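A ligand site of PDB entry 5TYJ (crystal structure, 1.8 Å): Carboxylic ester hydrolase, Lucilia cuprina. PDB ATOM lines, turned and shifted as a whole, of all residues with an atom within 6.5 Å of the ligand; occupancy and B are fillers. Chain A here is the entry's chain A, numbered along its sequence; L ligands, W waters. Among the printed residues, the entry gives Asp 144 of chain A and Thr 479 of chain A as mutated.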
ATOM      1  N   GLY A 142      12.655  10.700  28.163  1.00  0.00           N
ATOM      2  CA  GLY A 142      13.083  12.081  28.010  1.00  0.00           C
ATOM      3  C   GLY A 142      12.047  12.863  27.240  1.00  0.00           C
ATOM      4  O   GLY A 142      10.854  12.514  27.223  1.00  0.00           O
ATOM      5  N   GLY A 143      12.487  13.946  26.591  1.00  0.00           N
ATOM      6  CA  GLY A 143      11.556  14.875  25.981  1.00  0.00           C
ATOM      7  C   GLY A 143      11.660  16.281  26.568  1.00  0.00           C
ATOM      8  O   GLY A 143      10.672  17.041  26.585  1.00  0.00           O
ATOM      9  N   ASP A 144      12.861  16.615  27.043  1.00  0.00           N
ATOM     10  CA  ASP A 144      13.176  17.968  27.513  1.00  0.00           C
ATOM     11  C   ASP A 144      12.221  18.442  28.641  1.00  0.00           C
ATOM     12  O   ASP A 144      12.025  19.647  28.825  1.00  0.00           O
ATOM     13  CB  ASP A 144      13.134  18.934  26.308  1.00  0.00           C
ATOM     14  CG  ASP A 144      13.712  20.314  26.628  1.00  0.00           C
ATOM     15  OD1 ASP A 144      14.768  20.382  27.260  1.00  0.00           O
ATOM     16  OD2 ASP A 144      13.102  21.321  26.235  1.00  0.00           O
ATOM     17  N   PHE A 145      11.651  17.488  29.366  1.00  0.00           N
ATOM     18  CA  PHE A 145      10.653  17.741  30.439  1.00  0.00           C
ATOM     19  C   PHE A 145       9.393  18.416  29.930  1.00  0.00           C
ATOM     20  O   PHE A 145       8.597  18.929  30.737  1.00  0.00           O
ATOM     21  CB  PHE A 145      11.249  18.590  31.583  1.00  0.00           C
ATOM     22  CG  PHE A 145      12.397  17.938  32.311  1.00  0.00           C
ATOM     23  CD1 PHE A 145      12.176  16.890  33.213  1.00  0.00           C
ATOM     24  CD2 PHE A 145      13.700  18.349  32.089  1.00  0.00           C
ATOM     25  CE1 PHE A 145      13.238  16.286  33.877  1.00  0.00           C
ATOM     26  CE2 PHE A 145      14.768  17.756  32.747  1.00  0.00           C
ATOM     27  CZ  PHE A 145      14.538  16.714  33.638  1.00  0.00           C
ATOM     28  N   ILE A 146       9.187  18.441  28.608  1.00  0.00           N
ATOM     29  CA  ILE A 146       7.976  19.067  28.062  1.00  0.00           C
ATOM     30  C   ILE A 146       7.184  18.150  27.131  1.00  0.00           C
ATOM     31  O   ILE A 146       6.022  18.448  26.841  1.00  0.00           O
ATOM     32  CB  ILE A 146       8.322  20.404  27.298  1.00  0.00           C
ATOM     33  CG1 ILE A 146       9.225  20.160  26.087  1.00  0.00           C
ATOM     34  CG2 ILE A 146       8.980  21.426  28.247  1.00  0.00           C
ATOM     35  CD1 ILE A 146       9.445  21.428  25.255  1.00  0.00           C
ATOM     36  N   GLU A 224      16.754   8.237  29.110  1.00  0.00           N
ATOM     37  CA  GLU A 224      17.515   8.889  28.063  1.00  0.00           C
ATOM     38  C   GLU A 224      17.198  10.381  28.053  1.00  0.00           C
ATOM     39  O   GLU A 224      16.016  10.735  28.235  1.00  0.00           O
ATOM     40  CB  GLU A 224      17.182   8.239  26.709  1.00  0.00           C
ATOM     41  CG  GLU A 224      18.064   8.697  25.524  1.00  0.00           C
ATOM     42  CD  GLU A 224      17.423   9.821  24.759  1.00  0.00           C
ATOM     43  OE1 GLU A 224      16.241  10.071  25.029  1.00  0.00           O
ATOM     44  OE2 GLU A 224      18.103  10.461  23.905  1.00  0.00           O
ATOM     45  N   SER A 225      18.192  11.243  27.840  1.00  0.00           N
ATOM     46  CA  SER A 225      17.925  12.707  27.904  1.00  0.00           C
ATOM     47  C   SER A 225      17.422  13.236  29.221  1.00  0.00           C
ATOM     48  O   SER A 225      18.047  13.052  30.232  1.00  0.00           O
ATOM     49  CB  SER A 225      16.918  13.120  26.810  1.00  0.00           C
ATOM     50  OG  SER A 225      17.287  14.213  25.996  1.00  0.00           O
ATOM     51  N   ALA A 226      16.282  13.944  29.179  1.00  0.00           N
ATOM     52  CA  ALA A 226      15.672  14.425  30.415  1.00  0.00           C
ATOM     53  C   ALA A 226      15.395  13.223  31.340  1.00  0.00           C
ATOM     54  O   ALA A 226      15.338  13.372  32.563  1.00  0.00           O
ATOM     55  CB  ALA A 226      14.376  15.193  30.134  1.00  0.00           C
ATOM     56  N   GLY A 227      15.156  12.064  30.734  1.00  0.00           N
ATOM     57  CA  GLY A 227      15.001  10.806  31.433  1.00  0.00           C
ATOM     58  C   GLY A 227      16.279  10.331  32.092  1.00  0.00           C
ATOM     59  O   GLY A 227      16.235   9.695  33.140  1.00  0.00           O
ATOM     60  N   SER A 251      22.805   9.529  27.654  1.00  0.00           N
ATOM     61  CA  SER A 251      22.945  10.861  27.087  1.00  0.00           C
ATOM     62  C   SER A 251      22.343  11.942  27.980  1.00  0.00           C
ATOM     63  O   SER A 251      21.417  12.650  27.574  1.00  0.00           O
ATOM     64  CB  SER A 251      22.301  10.927  25.707  1.00  0.00           C
ATOM     65  OG  SER A 251      22.867   9.986  24.824  1.00  0.00           O
ATOM     66  N   TRP A 258      21.630  22.140  31.168  1.00  0.00           N
ATOM     67  CA  TRP A 258      20.247  22.177  30.754  1.00  0.00           C
ATOM     68  C   TRP A 258      19.317  21.451  31.724  1.00  0.00           C
ATOM     69  O   TRP A 258      18.114  21.533  31.569  1.00  0.00           O
ATOM     70  CB  TRP A 258      20.101  21.568  29.356  1.00  0.00           C
ATOM     71  CG  TRP A 258      20.707  20.180  29.219  1.00  0.00           C
ATOM     72  CD1 TRP A 258      21.983  19.862  28.757  1.00  0.00           C
ATOM     73  CD2 TRP A 258      20.067  18.915  29.506  1.00  0.00           C
ATOM     74  NE1 TRP A 258      22.153  18.495  28.767  1.00  0.00           N
ATOM     75  CE2 TRP A 258      21.001  17.894  29.224  1.00  0.00           C
ATOM     76  CE3 TRP A 258      18.806  18.552  29.987  1.00  0.00           C
ATOM     77  CZ2 TRP A 258      20.718  16.537  29.395  1.00  0.00           C
ATOM     78  CZ3 TRP A 258      18.515  17.204  30.171  1.00  0.00           C
ATOM     79  CH2 TRP A 258      19.480  16.209  29.879  1.00  0.00           C
ATOM     80  N   VAL A 314      19.174  28.288  27.948  1.00  0.00           N
ATOM     81  CA  VAL A 314      18.131  27.700  28.771  1.00  0.00           C
ATOM     82  C   VAL A 314      17.169  26.911  27.889  1.00  0.00           C
ATOM     83  O   VAL A 314      16.621  27.449  26.931  1.00  0.00           O
ATOM     84  CB  VAL A 314      17.366  28.808  29.541  1.00  0.00           C
ATOM     85  CG1 VAL A 314      16.354  28.211  30.502  1.00  0.00           C
ATOM     86  CG2 VAL A 314      18.357  29.680  30.272  1.00  0.00           C
ATOM     87  N   MET A 315      16.947  25.634  28.196  1.00  0.00           N
ATOM     88  CA  MET A 315      16.293  24.744  27.241  1.00  0.00           C
ATOM     89  C   MET A 315      14.810  24.529  27.518  1.00  0.00           C
ATOM     90  O   MET A 315      14.105  23.914  26.722  1.00  0.00           O
ATOM     91  CB  MET A 315      17.023  23.398  27.228  1.00  0.00           C
ATOM     92  CG  MET A 315      18.514  23.556  26.843  1.00  0.00           C
ATOM     93  SD  MET A 315      18.695  23.847  25.075  1.00  0.00           S
ATOM     94  CE  MET A 315      19.495  25.420  24.968  1.00  0.00           C
ATOM     95  N   PHE A 316      14.362  25.031  28.659  1.00  0.00           N
ATOM     96  CA  PHE A 316      12.951  24.975  29.021  1.00  0.00           C
ATOM     97  C   PHE A 316      12.658  26.026  30.070  1.00  0.00           C
ATOM     98  O   PHE A 316      13.518  26.355  30.877  1.00  0.00           O
ATOM     99  CB  PHE A 316      12.561  23.588  29.534  1.00  0.00           C
ATOM    100  CG  PHE A 316      13.545  22.998  30.514  1.00  0.00           C
ATOM    101  CD1 PHE A 316      13.640  23.471  31.805  1.00  0.00           C
ATOM    102  CD2 PHE A 316      14.391  21.975  30.124  1.00  0.00           C
ATOM    103  CE1 PHE A 316      14.553  22.937  32.716  1.00  0.00           C
ATOM    104  CE2 PHE A 316      15.280  21.432  31.018  1.00  0.00           C
ATOM    105  CZ  PHE A 316      15.376  21.912  32.321  1.00  0.00           C
ATOM    106  N   PHE A 361      21.316  15.953  16.507  1.00  0.00           N
ATOM    107  CA  PHE A 361      19.967  16.194  17.010  1.00  0.00           C
ATOM    108  C   PHE A 361      19.490  17.638  16.764  1.00  0.00           C
ATOM    109  O   PHE A 361      18.303  17.889  16.615  1.00  0.00           O
ATOM    110  CB  PHE A 361      19.941  15.871  18.511  1.00  0.00           C
ATOM    111  CG  PHE A 361      18.548  15.793  19.131  1.00  0.00           C
ATOM    112  CD1 PHE A 361      17.651  14.803  18.781  1.00  0.00           C
ATOM    113  CD2 PHE A 361      18.180  16.684  20.137  1.00  0.00           C
ATOM    114  CE1 PHE A 361      16.405  14.716  19.381  1.00  0.00           C
ATOM    115  CE2 PHE A 361      16.928  16.610  20.738  1.00  0.00           C
ATOM    116  CZ  PHE A 361      16.054  15.621  20.361  1.00  0.00           C
ATOM    117  N   PHE A 362      20.420  18.591  16.712  1.00  0.00           N
ATOM    118  CA  PHE A 362      20.027  20.004  16.648  1.00  0.00           C
ATOM    119  C   PHE A 362      19.883  20.517  15.213  1.00  0.00           C
ATOM    120  O   PHE A 362      19.686  21.706  14.996  1.00  0.00           O
ATOM    121  CB  PHE A 362      21.009  20.861  17.436  1.00  0.00           C
ATOM    122  CG  PHE A 362      20.989  20.581  18.897  1.00  0.00           C
ATOM    123  CD1 PHE A 362      19.923  20.983  19.674  1.00  0.00           C
ATOM    124  CD2 PHE A 362      22.023  19.885  19.501  1.00  0.00           C
ATOM    125  CE1 PHE A 362      19.889  20.706  21.039  1.00  0.00           C
ATOM    126  CE2 PHE A 362      21.998  19.604  20.866  1.00  0.00           C
ATOM    127  CZ  PHE A 362      20.937  20.018  21.637  1.00  0.00           C
ATOM    128  N   ILE A 365      16.569  22.572  14.531  1.00  0.00           N
ATOM    129  CA  ILE A 365      16.703  23.867  15.198  1.00  0.00           C
ATOM    130  C   ILE A 365      17.661  24.766  14.414  1.00  0.00           C
ATOM    131  O   ILE A 365      17.364  25.936  14.155  1.00  0.00           O
ATOM    132  CB  ILE A 365      17.217  23.714  16.640  1.00  0.00           C
ATOM    133  CG1 ILE A 365      16.053  23.469  17.586  1.00  0.00           C
ATOM    134  CG2 ILE A 365      17.948  24.973  17.077  1.00  0.00           C
ATOM    135  CD1 ILE A 365      15.247  24.744  17.903  1.00  0.00           C
ATOM    136  N   TYR A 427      26.379  19.910  25.625  1.00  0.00           N
ATOM    137  CA  TYR A 427      25.205  19.302  26.233  1.00  0.00           C
ATOM    138  C   TYR A 427      25.488  17.955  26.894  1.00  0.00           C
ATOM    139  O   TYR A 427      24.835  17.598  27.869  1.00  0.00           O
ATOM    140  CB  TYR A 427      24.091  19.148  25.203  1.00  0.00           C
ATOM    141  CG  TYR A 427      23.512  20.482  24.787  1.00  0.00           C
ATOM    142  CD1 TYR A 427      22.628  21.170  25.616  1.00  0.00           C
ATOM    143  CD2 TYR A 427      23.842  21.056  23.567  1.00  0.00           C
ATOM    144  CE1 TYR A 427      22.116  22.402  25.246  1.00  0.00           C
ATOM    145  CE2 TYR A 427      23.317  22.277  23.171  1.00  0.00           C
ATOM    146  CZ  TYR A 427      22.447  22.945  24.018  1.00  0.00           C
ATOM    147  OH  TYR A 427      21.918  24.159  23.651  1.00  0.00           O
ATOM    148  N   PHE A 428      26.456  17.201  26.394  1.00  0.00           N
ATOM    149  CA  PHE A 428      26.569  15.814  26.839  1.00  0.00           C
ATOM    150  C   PHE A 428      27.950  15.395  27.351  1.00  0.00           C
ATOM    151  O   PHE A 428      28.077  15.023  28.497  1.00  0.00           O
ATOM    152  CB  PHE A 428      26.109  14.870  25.712  1.00  0.00           C
ATOM    153  CG  PHE A 428      24.708  15.158  25.288  1.00  0.00           C
ATOM    154  CD1 PHE A 428      23.653  14.940  26.175  1.00  0.00           C
ATOM    155  CD2 PHE A 428      24.442  15.723  24.057  1.00  0.00           C
ATOM    156  CE1 PHE A 428      22.336  15.236  25.808  1.00  0.00           C
ATOM    157  CE2 PHE A 428      23.131  16.038  23.696  1.00  0.00           C
ATOM    158  CZ  PHE A 428      22.089  15.795  24.579  1.00  0.00           C
ATOM    159  N   TYR A 464      11.667  10.376  16.625  1.00  0.00           N
ATOM    160  CA  TYR A 464      12.483  11.547  16.905  1.00  0.00           C
ATOM    161  C   TYR A 464      13.452  11.835  15.751  1.00  0.00           C
ATOM    162  O   TYR A 464      14.033  12.909  15.677  1.00  0.00           O
ATOM    163  CB  TYR A 464      13.239  11.370  18.242  1.00  0.00           C
ATOM    164  CG  TYR A 464      12.283  11.431  19.427  1.00  0.00           C
ATOM    165  CD1 TYR A 464      11.099  12.152  19.319  1.00  0.00           C
ATOM    166  CD2 TYR A 464      12.534  10.753  20.615  1.00  0.00           C
ATOM    167  CE1 TYR A 464      10.188  12.223  20.357  1.00  0.00           C
ATOM    168  CE2 TYR A 464      11.620  10.822  21.695  1.00  0.00           C
ATOM    169  CZ  TYR A 464      10.446  11.565  21.541  1.00  0.00           C
ATOM    170  OH  TYR A 464       9.503  11.663  22.561  1.00  0.00           O
ATOM    171  N   MET A 467      11.791  14.706  14.067  1.00  0.00           N
ATOM    172  CA  MET A 467      12.100  15.887  14.878  1.00  0.00           C
ATOM    173  C   MET A 467      13.448  16.484  14.472  1.00  0.00           C
ATOM    174  O   MET A 467      13.552  17.680  14.230  1.00  0.00           O
ATOM    175  CB  MET A 467      12.117  15.539  16.379  1.00  0.00           C
ATOM    176  CG  MET A 467      13.162  16.285  17.241  1.00  0.00           C
ATOM    177  SD  MET A 467      13.034  18.089  17.302  1.00  0.00           S
ATOM    178  CE  MET A 467      14.346  18.495  18.440  1.00  0.00           C
ATOM    179  N   HIS A 478      21.694  12.048  19.005  1.00  0.00           N
ATOM    180  CA  HIS A 478      20.910  11.939  20.235  1.00  0.00           C
ATOM    181  C   HIS A 478      19.579  11.238  19.947  1.00  0.00           C
ATOM    182  O   HIS A 478      18.917  11.567  18.968  1.00  0.00           O
ATOM    183  CB  HIS A 478      20.667  13.354  20.813  1.00  0.00           C
ATOM    184  CG  HIS A 478      20.095  13.393  22.188  1.00  0.00           C
ATOM    185  ND1 HIS A 478      20.786  12.926  23.291  1.00  0.00           N
ATOM    186  CD2 HIS A 478      18.921  13.884  22.659  1.00  0.00           C
ATOM    187  CE1 HIS A 478      20.050  13.111  24.377  1.00  0.00           C
ATOM    188  NE2 HIS A 478      18.906  13.690  24.017  1.00  0.00           N
ATOM    189  N   THR A 479      19.211  10.246  20.788  1.00  0.00           N
ATOM    190  CA  THR A 479      17.968   9.429  20.671  1.00  0.00           C
ATOM    191  C   THR A 479      18.002   8.330  19.590  1.00  0.00           C
ATOM    192  O   THR A 479      17.042   7.564  19.467  1.00  0.00           O
ATOM    193  CB  THR A 479      16.647  10.242  20.377  1.00  0.00           C
ATOM    194  OG1 THR A 479      16.577  10.613  19.000  1.00  0.00           O
ATOM    195  CG2 THR A 479      16.522  11.474  21.270  1.00  0.00           C
HETATM  196 BR1  LIG L   1      19.806  19.165  25.441  1.00  0.00          BR
HETATM  197  C1  LIG L   1      18.147  18.420  24.902  1.00  0.00           C
HETATM  198  C2  LIG L   1      17.802  17.193  25.422  1.00  0.00           C
HETATM  199  C3  LIG L   1      16.602  16.607  25.049  1.00  0.00           C
HETATM  200  B1  LIG L   1      16.189  15.149  25.707  1.00  0.00           B
HETATM  201  O1  LIG L   1      15.044  14.410  24.789  1.00  0.00           O
HETATM  202  O2  LIG L   1      15.454  15.463  27.151  1.00  0.00           O
HETATM  203  C4  LIG L   1      15.758  17.252  24.168  1.00  0.00           C
HETATM  204  C5  LIG L   1      16.094  18.482  23.646  1.00  0.00           C
HETATM  205  O3  LIG L   1      15.177  19.068  22.749  1.00  0.00           O
HETATM  206  C6  LIG L   1      15.400  20.408  22.417  1.00  0.00           C
HETATM  207  C7  LIG L   1      15.785  20.699  21.131  1.00  0.00           C
HETATM  208  C8  LIG L   1      15.963  22.019  20.734  1.00  0.00           C
HETATM  209  C9  LIG L   1      15.732  23.044  21.661  1.00  0.00           C
HETATM  210  C10 LIG L   1      15.333  22.742  22.962  1.00  0.00           C
HETATM  211  C11 LIG L   1      15.154  21.418  23.337  1.00  0.00           C
HETATM  212  C12 LIG L   1      17.303  19.061  23.998  1.00  0.00           C
HETATM  213  O   HOH W   1      16.268  18.147  28.104  1.00  0.00           O
HETATM  214  O   HOH W   2      13.175  14.992  22.498  1.00  0.00           O
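A ring nitrogen (NE2) of His 478 lies within hydrogen-bond range of the side-chain hydroxyl of Ser 225, at 2.6 Å. O of Tyr 427 sits at hydrogen-bond distance from NE1 of Trp 258 (3.0 Å). SD of Met 315 lies close to OH of Tyr 427 (3.5 Å). The side-chain carboxylate of Glu 224 lies close to a ring nitrogen (NE2) of His 478 (3.3 Å).
The side-chain hydroxyl (OG) of Ser 225 is bonded to a boron (B1) of the ligand. O2 of the ligand is in hydrogen-bond range of N of Ala 226 (2.7 Å). O2 of the ligand sits at hydrogen-bond distance from N of Asp 144 (2.8 Å). N of Gly 143 sits at hydrogen-bond distance from O1 of the ligand, 3.2 Å away.
Residues that only touch the ligand: Phe 361 (3.6 Å), Ile 365 (3.5 Å), Tyr 427 (3.5 Å), Met 467 (3.8 Å) and His 478 (3.5 Å). Along chain A the residues within 4 Å of the ligand span positions 143 to 478.
Water W1 bridges OD1 of Asp 144 (2.8 Å) and O2 of the ligand (3.0 Å).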
